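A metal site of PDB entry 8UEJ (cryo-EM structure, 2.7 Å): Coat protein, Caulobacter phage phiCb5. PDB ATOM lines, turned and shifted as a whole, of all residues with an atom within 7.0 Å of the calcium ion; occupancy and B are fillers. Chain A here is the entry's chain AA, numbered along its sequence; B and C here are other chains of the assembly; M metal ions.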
ATOM      1  N   ASN A  24      19.527   2.958  21.671  1.00  0.00           N
ATOM      2  CA  ASN A  24      19.259   1.546  21.487  1.00  0.00           C
ATOM      3  C   ASN A  24      20.575   0.773  21.535  1.00  0.00           C
ATOM      4  O   ASN A  24      21.647   1.352  21.717  1.00  0.00           O
ATOM      5  CB  ASN A  24      18.521   1.280  20.161  1.00  0.00           C
ATOM      6  CG  ASN A  24      19.345   1.651  18.936  1.00  0.00           C
ATOM      7  OD1 ASN A  24      20.516   2.007  19.042  1.00  0.00           O
ATOM      8  ND2 ASN A  24      18.736   1.518  17.770  1.00  0.00           N
ATOM      9  N   GLN A  25      20.468  -0.551  21.396  1.00  0.00           N
ATOM     10  CA  GLN A  25      21.639  -1.419  21.353  1.00  0.00           C
ATOM     11  C   GLN A  25      21.279  -2.620  20.486  1.00  0.00           C
ATOM     12  O   GLN A  25      20.682  -3.576  20.978  1.00  0.00           O
ATOM     13  CB  GLN A  25      22.072  -1.845  22.746  1.00  0.00           C
ATOM     14  CG  GLN A  25      23.494  -2.413  22.826  1.00  0.00           C
ATOM     15  CD  GLN A  25      23.573  -3.872  22.421  1.00  0.00           C
ATOM     16  OE1 GLN A  25      22.629  -4.637  22.634  1.00  0.00           O
ATOM     17  NE2 GLN A  25      24.699  -4.266  21.834  1.00  0.00           N
ATOM     18  N   ASP A  26      21.656  -2.575  19.208  1.00  0.00           N
ATOM     19  CA  ASP A  26      21.368  -3.646  18.270  1.00  0.00           C
ATOM     20  C   ASP A  26      22.632  -4.074  17.536  1.00  0.00           C
ATOM     21  O   ASP A  26      23.452  -3.234  17.147  1.00  0.00           O
ATOM     22  CB  ASP A  26      20.323  -3.229  17.224  1.00  0.00           C
ATOM     23  CG  ASP A  26      18.948  -3.031  17.807  1.00  0.00           C
ATOM     24  OD1 ASP A  26      18.630  -3.707  18.812  1.00  0.00           O
ATOM     25  OD2 ASP A  26      18.183  -2.228  17.254  1.00  0.00           O
ATOM     26  N   GLY A  27      22.769  -5.381  17.343  1.00  0.00           N
ATOM     27  CA  GLY A  27      23.831  -5.914  16.514  1.00  0.00           C
ATOM     28  C   GLY A  27      25.228  -5.550  16.973  1.00  0.00           C
ATOM     29  O   GLY A  27      26.088  -5.245  16.147  1.00  0.00           O
ATOM     30  N   ASN B  24      13.092  -6.377  26.951  1.00  0.00           N
ATOM     31  CA  ASN B  24      13.613  -6.216  25.602  1.00  0.00           C
ATOM     32  C   ASN B  24      13.591  -4.749  25.187  1.00  0.00           C
ATOM     33  O   ASN B  24      12.786  -3.964  25.703  1.00  0.00           O
ATOM     34  CB  ASN B  24      12.810  -7.050  24.588  1.00  0.00           C
ATOM     35  CG  ASN B  24      13.340  -6.904  23.170  1.00  0.00           C
ATOM     36  OD1 ASN B  24      14.381  -6.297  22.957  1.00  0.00           O
ATOM     37  ND2 ASN B  24      12.605  -7.435  22.203  1.00  0.00           N
ATOM     38  N   GLN B  25      14.492  -4.403  24.264  1.00  0.00           N
ATOM     39  CA  GLN B  25      14.433  -3.121  23.558  1.00  0.00           C
ATOM     40  C   GLN B  25      15.325  -3.229  22.326  1.00  0.00           C
ATOM     41  O   GLN B  25      16.535  -3.392  22.470  1.00  0.00           O
ATOM     42  CB  GLN B  25      14.871  -1.969  24.462  1.00  0.00           C
ATOM     43  CG  GLN B  25      16.325  -2.012  24.890  1.00  0.00           C
ATOM     44  CD  GLN B  25      16.691  -0.885  25.827  1.00  0.00           C
ATOM     45  OE1 GLN B  25      15.874  -0.009  26.122  1.00  0.00           O
ATOM     46  NE2 GLN B  25      17.941  -0.890  26.293  1.00  0.00           N
ATOM     47  N   ASP B  26      14.734  -3.152  21.124  1.00  0.00           N
ATOM     48  CA  ASP B  26      15.522  -3.237  19.899  1.00  0.00           C
ATOM     49  C   ASP B  26      15.383  -2.015  19.003  1.00  0.00           C
ATOM     50  O   ASP B  26      16.383  -1.340  18.727  1.00  0.00           O
ATOM     51  CB  ASP B  26      15.121  -4.500  19.137  1.00  0.00           C
ATOM     52  CG  ASP B  26      15.254  -5.755  19.983  1.00  0.00           C
ATOM     53  OD1 ASP B  26      16.165  -5.799  20.831  1.00  0.00           O
ATOM     54  OD2 ASP B  26      14.442  -6.691  19.801  1.00  0.00           O
ATOM     55  N   GLY B  27      14.173  -1.677  18.555  1.00  0.00           N
ATOM     56  CA  GLY B  27      14.017  -0.650  17.537  1.00  0.00           C
ATOM     57  C   GLY B  27      13.644   0.708  18.080  1.00  0.00           C
ATOM     58  O   GLY B  27      12.608   1.258  17.719  1.00  0.00           O
ATOM     59  N   THR B  29      12.655   1.082  20.903  1.00  0.00           N
ATOM     60  CA  THR B  29      11.495   0.779  21.720  1.00  0.00           C
ATOM     61  C   THR B  29      11.923  -0.124  22.870  1.00  0.00           C
ATOM     62  O   THR B  29      12.938  -0.820  22.775  1.00  0.00           O
ATOM     63  CB  THR B  29      10.400   0.076  20.917  1.00  0.00           C
ATOM     64  OG1 THR B  29      10.841  -1.249  20.572  1.00  0.00           O
ATOM     65  CG2 THR B  29      10.127   0.827  19.637  1.00  0.00           C
ATOM     66  N   ASN C  24      25.318  -7.551  24.238  1.00  0.00           N
ATOM     67  CA  ASN C  24      24.205  -7.451  23.303  1.00  0.00           C
ATOM     68  C   ASN C  24      22.912  -7.868  23.999  1.00  0.00           C
ATOM     69  O   ASN C  24      22.945  -8.620  24.973  1.00  0.00           O
ATOM     70  CB  ASN C  24      24.436  -8.336  22.068  1.00  0.00           C
ATOM     71  CG  ASN C  24      23.985  -7.679  20.789  1.00  0.00           C
ATOM     72  OD1 ASN C  24      23.925  -6.451  20.685  1.00  0.00           O
ATOM     73  ND2 ASN C  24      23.648  -8.498  19.796  1.00  0.00           N
ATOM     74  N   GLN C  25      21.791  -7.359  23.487  1.00  0.00           N
ATOM     75  CA  GLN C  25      20.481  -7.865  23.884  1.00  0.00           C
ATOM     76  C   GLN C  25      19.519  -7.607  22.717  1.00  0.00           C
ATOM     77  O   GLN C  25      19.047  -6.475  22.540  1.00  0.00           O
ATOM     78  CB  GLN C  25      19.981  -7.217  25.169  1.00  0.00           C
ATOM     79  CG  GLN C  25      18.720  -7.874  25.689  1.00  0.00           C
ATOM     80  CD  GLN C  25      17.455  -7.330  25.073  1.00  0.00           C
ATOM     81  OE1 GLN C  25      17.384  -6.162  24.685  1.00  0.00           O
ATOM     82  NE2 GLN C  25      16.450  -8.194  24.931  1.00  0.00           N
ATOM     83  N   ASP C  26      19.239  -8.648  21.950  1.00  0.00           N
ATOM     84  CA  ASP C  26      18.337  -8.567  20.808  1.00  0.00           C
ATOM     85  C   ASP C  26      17.369  -9.743  20.830  1.00  0.00           C
ATOM     86  O   ASP C  26      17.765 -10.867  21.160  1.00  0.00           O
ATOM     87  CB  ASP C  26      19.102  -8.578  19.472  1.00  0.00           C
ATOM     88  CG  ASP C  26      19.751  -7.255  19.156  1.00  0.00           C
ATOM     89  OD1 ASP C  26      19.549  -6.288  19.919  1.00  0.00           O
ATOM     90  OD2 ASP C  26      20.475  -7.177  18.144  1.00  0.00           O
ATOM     91  N   GLY C  27      16.123  -9.483  20.482  1.00  0.00           N
ATOM     92  CA  GLY C  27      15.128 -10.538  20.338  1.00  0.00           C
ATOM     93  C   GLY C  27      14.913 -11.374  21.575  1.00  0.00           C
ATOM     94  O   GLY C  27      14.867 -12.603  21.502  1.00  0.00           O
HETATM   95 CA    CA M   1      18.567  -4.197  21.638  1.00  0.00          CA
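NE2 of Gln 25 of chain A is in hydrogen-bond range of OD1 of Asn 24 of chain C (2.6 Å).
The side-chain amide oxygen of Asn 24 of chain B is in hydrogen-bond range of the side-chain amide nitrogen of Gln 25 of chain C (3.4 Å).
OD2 of Asp 26 of chain A sits close to O of Asp 26 of chain B (2.5 Å).
OD2 of Asp 26 of chain C lies within hydrogen-bond range of N of Gly 27 of chain A, at 3.0 Å.
The side-chain carboxylate of Asp 26 of chain B sits close to the side-chain amide oxygen of Asn 24 of chain B (2.8 Å).
N of Gly 27 of chain C is in hydrogen-bond range of OD2 of Asp 26 of chain B (3.3 Å).
Along chain A the residues within 4 Å of the calcium ion span positions 25 to 26.
The calcium ion is bound by O of Gln 25 of chain A (2.3 Å), O of Gln 25 of chain B (2.3 Å), O of Gln 25 of chain C (2.5 Å), OD1 of Asp 26 of chain A (2.9 Å) and OD1 of Asp 26 of chain C (2.9 Å).
Slightly farther from the calcium ion lies OD1 of Asp 26 of chain B (3.0 Å).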
